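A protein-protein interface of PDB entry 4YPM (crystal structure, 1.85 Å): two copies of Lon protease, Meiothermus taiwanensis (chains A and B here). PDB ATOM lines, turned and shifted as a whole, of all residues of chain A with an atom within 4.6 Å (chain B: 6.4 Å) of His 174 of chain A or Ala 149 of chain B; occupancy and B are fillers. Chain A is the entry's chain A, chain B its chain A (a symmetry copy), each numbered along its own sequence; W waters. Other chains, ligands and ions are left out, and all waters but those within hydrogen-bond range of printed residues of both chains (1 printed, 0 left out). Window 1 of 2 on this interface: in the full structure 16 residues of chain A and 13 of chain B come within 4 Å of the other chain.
OG of Ser 217 of chain B lies within hydrogen-bond range of OE2 of Glu 123 of chain A, at 2.7 Å. The backbone NH (N) of Leu 218 of chain B is in hydrogen-bond range of the side-chain carboxylate (OE1) of Glu 123 of chain A, 2.8 Å away. ND1 of His 174 of chain A sits at hydrogen-bond distance from OG1 of Thr 152 of chain B (2.8 Å).
Hydrophobic or aromatic side chains of chain A that line the printed part of chain B: Ala 125, His 174 and His 176. Printed residues of chain B that touch a printed residue of chain A: Glu 145, Gln 148, Ala 149, Thr 152, Ser 217 and Leu 218. Hydrophobic or aromatic side chains of chain B that line the printed part of chain A: Leu 218. Along chain B the printed residues that touch a printed residue of chain A span positions 145 to 218. Among the printed residues, no Asp or Glu carboxylate lies within 4 Å of a Lys or Arg side-chain nitrogen of the other chain.
The backbone carbonyl oxygen (O) of Glu 123 of chain A is in hydrogen-bond range of the backbone NH (N) of His 176 of chain A. N of Ala 125 of chain A lies within hydrogen-bond range of O of His 174 of chain A, at 3.0 Å. NE2 of His 174 of chain A lies within hydrogen-bond range of OG1 of Thr 136 of chain A, 2.7 Å away. N of Thr 136 of chain A lies within hydrogen-bond range of O of Val 175 of chain A, at 2.8 Å. OG1 of Thr 136 of chain A lies within hydrogen-bond range of ND1 of His 176 of chain A (2.7 Å). O of Gln 148 of chain B is in hydrogen-bond range of OG1 of Thr 152 of chain B, at 3.3 Å.
No position is printed for both chains.
Water W1 lies within hydrogen-bond range of O of Val 216 of chain B (2.8 Å) and NE2 of His 176 of chain A (2.8 Å).
Among the printed residues, merely in contact across the chains: Ala 125 of chain A with Thr 152 of chain B, Ala 125 of chain A with Leu 218 of chain B, Thr 136 of chain A with Glu 145 of chain B, Thr 136 of chain A with Gln 148 of chain B, His 174 of chain A with Gln 148 of chain B, His 174 of chain A with Ala 149 of chain B, His 174 of chain A with Leu 218 of chain B and His 176 of chain A with Leu 218 of chain B.
His 174 of chain A touches just these residues of chain B: Gln 148 (3.7 Å), Ala 149 (3.9 Å), Thr 152 (2.8 Å) and Leu 218 (3.3 Å). Ala 149 of chain B touches just one residue of chain A: His 174. Of the printed residues of chain A, Thr 152 of chain B touches Ala 125 (3.5 Å) and His 174 (2.8 Å). Of the printed residues of chain B, Thr 136 of chain A touches Glu 145 (3.7 Å) and Gln 148 (3.7 Å). Of the printed residues of chain B, His 176 of chain A touches Leu 218 (3.9 Å). Of the printed residues of chain B, Glu 123 of chain A touches Ser 217 (2.7 Å) and Leu 218 (2.8 Å). Asp 172 of chain A touches none of the printed residues of chain B. The nearest printed residue of chain A that does not touch Ala 149 of chain B is His 176 of chain A (4.6 Å).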
ATOM      1  N   GLU A 123       7.534 -17.757   9.592  1.00  0.00           N
ATOM      2  CA  GLU A 123       8.041 -17.639   8.218  1.00  0.00           C
ATOM      3  C   GLU A 123       7.673 -16.282   7.639  1.00  0.00           C
ATOM      4  O   GLU A 123       6.545 -15.817   7.819  1.00  0.00           O
ATOM      5  CB  GLU A 123       7.437 -18.706   7.320  1.00  0.00           C
ATOM      6  CG  GLU A 123       7.648 -20.135   7.742  1.00  0.00           C
ATOM      7  CD  GLU A 123       7.012 -21.070   6.744  1.00  0.00           C
ATOM      8  OE1 GLU A 123       5.774 -21.036   6.616  1.00  0.00           O
ATOM      9  OE2 GLU A 123       7.749 -21.800   6.032  1.00  0.00           O
ATOM     10  N   VAL A 124       8.622 -15.644   6.947  1.00  0.00           N
ATOM     11  CA  VAL A 124       8.377 -14.379   6.284  1.00  0.00           C
ATOM     12  C   VAL A 124       8.992 -14.422   4.887  1.00  0.00           C
ATOM     13  O   VAL A 124      10.141 -14.823   4.717  1.00  0.00           O
ATOM     14  CB  VAL A 124       8.969 -13.188   7.054  1.00  0.00           C
ATOM     15  CG1 VAL A 124       8.698 -11.860   6.340  1.00  0.00           C
ATOM     16  CG2 VAL A 124       8.384 -13.135   8.449  1.00  0.00           C
ATOM     17  N   ALA A 125       8.197 -14.006   3.908  1.00  0.00           N
ATOM     18  CA  ALA A 125       8.670 -13.758   2.556  1.00  0.00           C
ATOM     19  C   ALA A 125       8.631 -12.273   2.246  1.00  0.00           C
ATOM     20  O   ALA A 125       7.671 -11.539   2.611  1.00  0.00           O
ATOM     21  CB  ALA A 125       7.816 -14.516   1.550  1.00  0.00           C
ATOM     22  N   SER A 134       0.673  -9.252   4.325  1.00  0.00           N
ATOM     23  CA  SER A 134      -0.235 -10.358   4.580  1.00  0.00           C
ATOM     24  C   SER A 134       0.201 -11.070   5.859  1.00  0.00           C
ATOM     25  O   SER A 134       1.385 -11.263   6.090  1.00  0.00           O
ATOM     26  CB  SER A 134      -0.221 -11.341   3.397  1.00  0.00           C
ATOM     27  OG  SER A 134      -0.603 -10.665   2.204  1.00  0.00           O
ATOM     28  N   THR A 136      -0.826 -14.516   7.941  1.00  0.00           N
ATOM     29  CA  THR A 136      -1.605 -15.731   7.829  1.00  0.00           C
ATOM     30  C   THR A 136      -1.138 -16.803   8.809  1.00  0.00           C
ATOM     31  O   THR A 136      -0.075 -16.682   9.439  1.00  0.00           O
ATOM     32  CB  THR A 136      -1.613 -16.290   6.384  1.00  0.00           C
ATOM     33  OG1 THR A 136      -0.275 -16.618   5.966  1.00  0.00           O
ATOM     34  CG2 THR A 136      -2.230 -15.283   5.406  1.00  0.00           C
ATOM     35  N   ASP A 172       6.363  -6.395  -1.015  1.00  0.00           N
ATOM     36  CA  ASP A 172       5.265  -6.945  -0.211  1.00  0.00           C
ATOM     37  C   ASP A 172       5.829  -7.959   0.760  1.00  0.00           C
ATOM     38  O   ASP A 172       6.745  -8.730   0.426  1.00  0.00           O
ATOM     39  CB  ASP A 172       4.183  -7.622  -1.068  1.00  0.00           C
ATOM     40  CG  ASP A 172       3.353  -6.648  -1.870  1.00  0.00           C
ATOM     41  OD1 ASP A 172       3.470  -5.411  -1.676  1.00  0.00           O
ATOM     42  OD2 ASP A 172       2.555  -7.145  -2.737  1.00  0.00           O
ATOM     43  N   LEU A 173       5.288  -7.939   1.980  1.00  0.00           N
ATOM     44  CA  LEU A 173       5.684  -8.872   3.010  1.00  0.00           C
ATOM     45  C   LEU A 173       4.534  -9.823   3.300  1.00  0.00           C
ATOM     46  O   LEU A 173       3.363  -9.437   3.274  1.00  0.00           O
ATOM     47  CB  LEU A 173       6.097  -8.124   4.279  1.00  0.00           C
ATOM     48  CG  LEU A 173       7.482  -7.467   4.215  1.00  0.00           C
ATOM     49  CD1 LEU A 173       7.587  -6.422   5.296  1.00  0.00           C
ATOM     50  CD2 LEU A 173       8.580  -8.511   4.356  1.00  0.00           C
ATOM     51  N   HIS A 174       4.879 -11.059   3.609  1.00  0.00           N
ATOM     52  CA  HIS A 174       3.909 -12.059   4.013  1.00  0.00           C
ATOM     53  C   HIS A 174       4.507 -12.792   5.223  1.00  0.00           C
ATOM     54  O   HIS A 174       5.585 -13.381   5.136  1.00  0.00           O
ATOM     55  CB  HIS A 174       3.639 -13.024   2.861  1.00  0.00           C
ATOM     56  CG  HIS A 174       2.521 -13.988   3.120  1.00  0.00           C
ATOM     57  ND1 HIS A 174       1.809 -14.586   2.101  1.00  0.00           N
ATOM     58  CD2 HIS A 174       1.980 -14.451   4.275  1.00  0.00           C
ATOM     59  CE1 HIS A 174       0.894 -15.392   2.615  1.00  0.00           C
ATOM     60  NE2 HIS A 174       0.973 -15.321   3.931  1.00  0.00           N
ATOM     61  N   VAL A 175       3.811 -12.697   6.352  1.00  0.00           N
ATOM     62  CA  VAL A 175       4.186 -13.392   7.587  1.00  0.00           C
ATOM     63  C   VAL A 175       3.224 -14.552   7.718  1.00  0.00           C
ATOM     64  O   VAL A 175       2.006 -14.348   7.699  1.00  0.00           O
ATOM     65  CB  VAL A 175       4.042 -12.495   8.848  1.00  0.00           C
ATOM     66  CG1 VAL A 175       4.464 -13.265  10.108  1.00  0.00           C
ATOM     67  CG2 VAL A 175       4.844 -11.205   8.715  1.00  0.00           C
ATOM     68  N   HIS A 176       3.748 -15.764   7.848  1.00  0.00           N
ATOM     69  CA  HIS A 176       2.941 -16.951   7.982  1.00  0.00           C
ATOM     70  C   HIS A 176       3.467 -17.800   9.128  1.00  0.00           C
ATOM     71  O   HIS A 176       4.681 -17.988   9.275  1.00  0.00           O
ATOM     72  CB  HIS A 176       2.959 -17.756   6.687  1.00  0.00           C
ATOM     73  CG  HIS A 176       2.121 -18.993   6.721  1.00  0.00           C
ATOM     74  ND1 HIS A 176       0.745 -18.959   6.722  1.00  0.00           N
ATOM     75  CD2 HIS A 176       2.465 -20.298   6.729  1.00  0.00           C
ATOM     76  CE1 HIS A 176       0.276 -20.190   6.745  1.00  0.00           C
ATOM     77  NE2 HIS A 176       1.301 -21.024   6.754  1.00  0.00           N
ATOM     78  N   LYS B 144      -8.369 -20.312   2.100  1.00  0.00           N
ATOM     79  CA  LYS B 144      -7.956 -19.087   1.423  1.00  0.00           C
ATOM     80  C   LYS B 144      -6.537 -18.667   1.794  1.00  0.00           C
ATOM     81  O   LYS B 144      -5.766 -18.221   0.920  1.00  0.00           O
ATOM     82  CB  LYS B 144      -8.940 -17.964   1.653  1.00  0.00           C
ATOM     83  CG  LYS B 144     -10.240 -18.186   0.915  1.00  0.00           C
ATOM     84  CD  LYS B 144     -11.105 -16.949   1.063  1.00  0.00           C
ATOM     85  CE  LYS B 144     -12.419 -17.039   0.324  1.00  0.00           C
ATOM     86  NZ  LYS B 144     -13.285 -15.933   0.857  1.00  0.00           N
ATOM     87  N   GLU B 145      -6.177 -18.798   3.068  1.00  0.00           N
ATOM     88  CA  GLU B 145      -4.810 -18.473   3.516  1.00  0.00           C
ATOM     89  C   GLU B 145      -3.784 -19.424   2.879  1.00  0.00           C
ATOM     90  O   GLU B 145      -2.673 -19.021   2.552  1.00  0.00           O
ATOM     91  CB  GLU B 145      -4.700 -18.489   5.051  1.00  0.00           C
ATOM     92  CG  GLU B 145      -5.452 -17.339   5.716  1.00  0.00           C
ATOM     93  CD  GLU B 145      -5.157 -17.147   7.196  1.00  0.00           C
ATOM     94  OE1 GLU B 145      -4.589 -18.033   7.882  1.00  0.00           O
ATOM     95  OE2 GLU B 145      -5.518 -16.058   7.682  1.00  0.00           O
ATOM     96  N   SER B 146      -4.186 -20.674   2.690  1.00  0.00           N
ATOM     97  CA  SER B 146      -3.370 -21.672   2.030  1.00  0.00           C
ATOM     98  C   SER B 146      -3.059 -21.242   0.595  1.00  0.00           C
ATOM     99  O   SER B 146      -1.916 -21.360   0.138  1.00  0.00           O
ATOM    100  CB  SER B 146      -4.100 -23.003   2.059  1.00  0.00           C
ATOM    101  OG  SER B 146      -3.475 -23.957   1.272  1.00  0.00           O
ATOM    102  N   ALA B 147      -4.073 -20.748  -0.112  1.00  0.00           N
ATOM    103  CA  ALA B 147      -3.858 -20.216  -1.472  1.00  0.00           C
ATOM    104  C   ALA B 147      -2.887 -19.038  -1.471  1.00  0.00           C
ATOM    105  O   ALA B 147      -2.015 -18.924  -2.350  1.00  0.00           O
ATOM    106  CB  ALA B 147      -5.163 -19.809  -2.101  1.00  0.00           C
ATOM    107  N   GLN B 148      -3.033 -18.160  -0.487  1.00  0.00           N
ATOM    108  CA  GLN B 148      -2.148 -17.017  -0.363  1.00  0.00           C
ATOM    109  C   GLN B 148      -0.699 -17.458  -0.107  1.00  0.00           C
ATOM    110  O   GLN B 148       0.222 -16.906  -0.692  1.00  0.00           O
ATOM    111  CB  GLN B 148      -2.612 -16.078   0.738  1.00  0.00           C
ATOM    112  CG  GLN B 148      -3.937 -15.388   0.465  1.00  0.00           C
ATOM    113  CD  GLN B 148      -4.264 -14.400   1.559  1.00  0.00           C
ATOM    114  OE1 GLN B 148      -4.017 -13.193   1.421  1.00  0.00           O
ATOM    115  NE2 GLN B 148      -4.724 -14.890   2.659  1.00  0.00           N
ATOM    116  N   ALA B 149      -0.512 -18.472   0.747  1.00  0.00           N
ATOM    117  CA  ALA B 149       0.834 -18.970   1.034  1.00  0.00           C
ATOM    118  C   ALA B 149       1.469 -19.584  -0.218  1.00  0.00           C
ATOM    119  O   ALA B 149       2.637 -19.321  -0.522  1.00  0.00           O
ATOM    120  CB  ALA B 149       0.802 -19.990   2.145  1.00  0.00           C
ATOM    121  N   ALA B 150       0.687 -20.369  -0.951  1.00  0.00           N
ATOM    122  CA  ALA B 150       1.151 -20.950  -2.222  1.00  0.00           C
ATOM    123  C   ALA B 150       1.570 -19.860  -3.218  1.00  0.00           C
ATOM    124  O   ALA B 150       2.641 -19.945  -3.835  1.00  0.00           O
ATOM    125  CB  ALA B 150       0.085 -21.850  -2.822  1.00  0.00           C
ATOM    126  N   LEU B 151       0.756 -18.819  -3.339  1.00  0.00           N
ATOM    127  CA  LEU B 151       1.039 -17.737  -4.287  1.00  0.00           C
ATOM    128  C   LEU B 151       2.302 -16.967  -3.905  1.00  0.00           C
ATOM    129  O   LEU B 151       3.156 -16.641  -4.752  1.00  0.00           O
ATOM    130  CB  LEU B 151      -0.177 -16.820  -4.406  1.00  0.00           C
ATOM    131  CG  LEU B 151      -0.053 -15.585  -5.301  1.00  0.00           C
ATOM    132  CD1 LEU B 151       0.439 -15.937  -6.693  1.00  0.00           C
ATOM    133  CD2 LEU B 151      -1.379 -14.835  -5.389  1.00  0.00           C
ATOM    134  N   THR B 152       2.454 -16.701  -2.619  1.00  0.00           N
ATOM    135  CA  THR B 152       3.651 -16.024  -2.147  1.00  0.00           C
ATOM    136  C   THR B 152       4.920 -16.842  -2.389  1.00  0.00           C
ATOM    137  O   THR B 152       5.924 -16.281  -2.814  1.00  0.00           O
ATOM    138  CB  THR B 152       3.535 -15.607  -0.676  1.00  0.00           C
ATOM    139  OG1 THR B 152       2.580 -14.543  -0.590  1.00  0.00           O
ATOM    140  CG2 THR B 152       4.862 -15.125  -0.145  1.00  0.00           C
ATOM    141  N   TYR B 153       4.858 -18.147  -2.143  1.00  0.00           N
ATOM    142  CA  TYR B 153       5.952 -19.035  -2.453  1.00  0.00           C
ATOM    143  C   TYR B 153       6.338 -18.872  -3.942  1.00  0.00           C
ATOM    144  O   TYR B 153       7.519 -18.714  -4.295  1.00  0.00           O
ATOM    145  CB  TYR B 153       5.594 -20.493  -2.128  1.00  0.00           C
ATOM    146  CG  TYR B 153       6.643 -21.443  -2.638  1.00  0.00           C
ATOM    147  CD1 TYR B 153       7.792 -21.704  -1.897  1.00  0.00           C
ATOM    148  CD2 TYR B 153       6.537 -22.000  -3.903  1.00  0.00           C
ATOM    149  CE1 TYR B 153       8.786 -22.551  -2.387  1.00  0.00           C
ATOM    150  CE2 TYR B 153       7.524 -22.832  -4.402  1.00  0.00           C
ATOM    151  CZ  TYR B 153       8.647 -23.104  -3.639  1.00  0.00           C
ATOM    152  OH  TYR B 153       9.616 -23.941  -4.155  1.00  0.00           O
ATOM    153  N   LEU B 154       5.343 -18.866  -4.811  1.00  0.00           N
ATOM    154  CA  LEU B 154       5.618 -18.725  -6.255  1.00  0.00           C
ATOM    155  C   LEU B 154       6.172 -17.361  -6.633  1.00  0.00           C
ATOM    156  O   LEU B 154       7.097 -17.268  -7.445  1.00  0.00           O
ATOM    157  CB  LEU B 154       4.398 -19.060  -7.078  1.00  0.00           C
ATOM    158  CG  LEU B 154       3.922 -20.503  -6.934  1.00  0.00           C
ATOM    159  CD1 LEU B 154       2.596 -20.684  -7.625  1.00  0.00           C
ATOM    160  CD2 LEU B 154       4.925 -21.509  -7.469  1.00  0.00           C
ATOM    161  N   VAL B 216       1.179 -26.706   2.557  1.00  0.00           N
ATOM    162  CA  VAL B 216       2.426 -26.037   2.183  1.00  0.00           C
ATOM    163  C   VAL B 216       2.748 -24.936   3.195  1.00  0.00           C
ATOM    164  O   VAL B 216       1.862 -24.214   3.643  1.00  0.00           O
ATOM    165  CB  VAL B 216       2.360 -25.516   0.724  1.00  0.00           C
ATOM    166  CG1 VAL B 216       1.507 -24.261   0.612  1.00  0.00           C
ATOM    167  CG2 VAL B 216       3.767 -25.295   0.171  1.00  0.00           C
ATOM    168  N   SER B 217       4.014 -24.841   3.583  1.00  0.00           N
ATOM    169  CA  SER B 217       4.483 -23.698   4.358  1.00  0.00           C
ATOM    170  C   SER B 217       4.898 -22.609   3.386  1.00  0.00           C
ATOM    171  O   SER B 217       5.067 -22.845   2.174  1.00  0.00           O
ATOM    172  CB  SER B 217       5.638 -24.097   5.275  1.00  0.00           C
ATOM    173  OG  SER B 217       6.901 -24.011   4.634  1.00  0.00           O
ATOM    174  N   LEU B 218       5.112 -21.417   3.922  1.00  0.00           N
ATOM    175  CA  LEU B 218       5.489 -20.302   3.100  1.00  0.00           C
ATOM    176  C   LEU B 218       6.787 -20.522   2.348  1.00  0.00           C
ATOM    177  O   LEU B 218       6.930 -20.045   1.218  1.00  0.00           O
ATOM    178  CB  LEU B 218       5.571 -19.030   3.934  1.00  0.00           C
ATOM    179  CG  LEU B 218       5.484 -17.728   3.190  1.00  0.00           C
ATOM    180  CD1 LEU B 218       4.167 -17.644   2.454  1.00  0.00           C
ATOM    181  CD2 LEU B 218       5.656 -16.556   4.141  1.00  0.00           C
HETATM  182  O   HOH W   1       0.820 -23.727   6.182  1.00  0.00           O
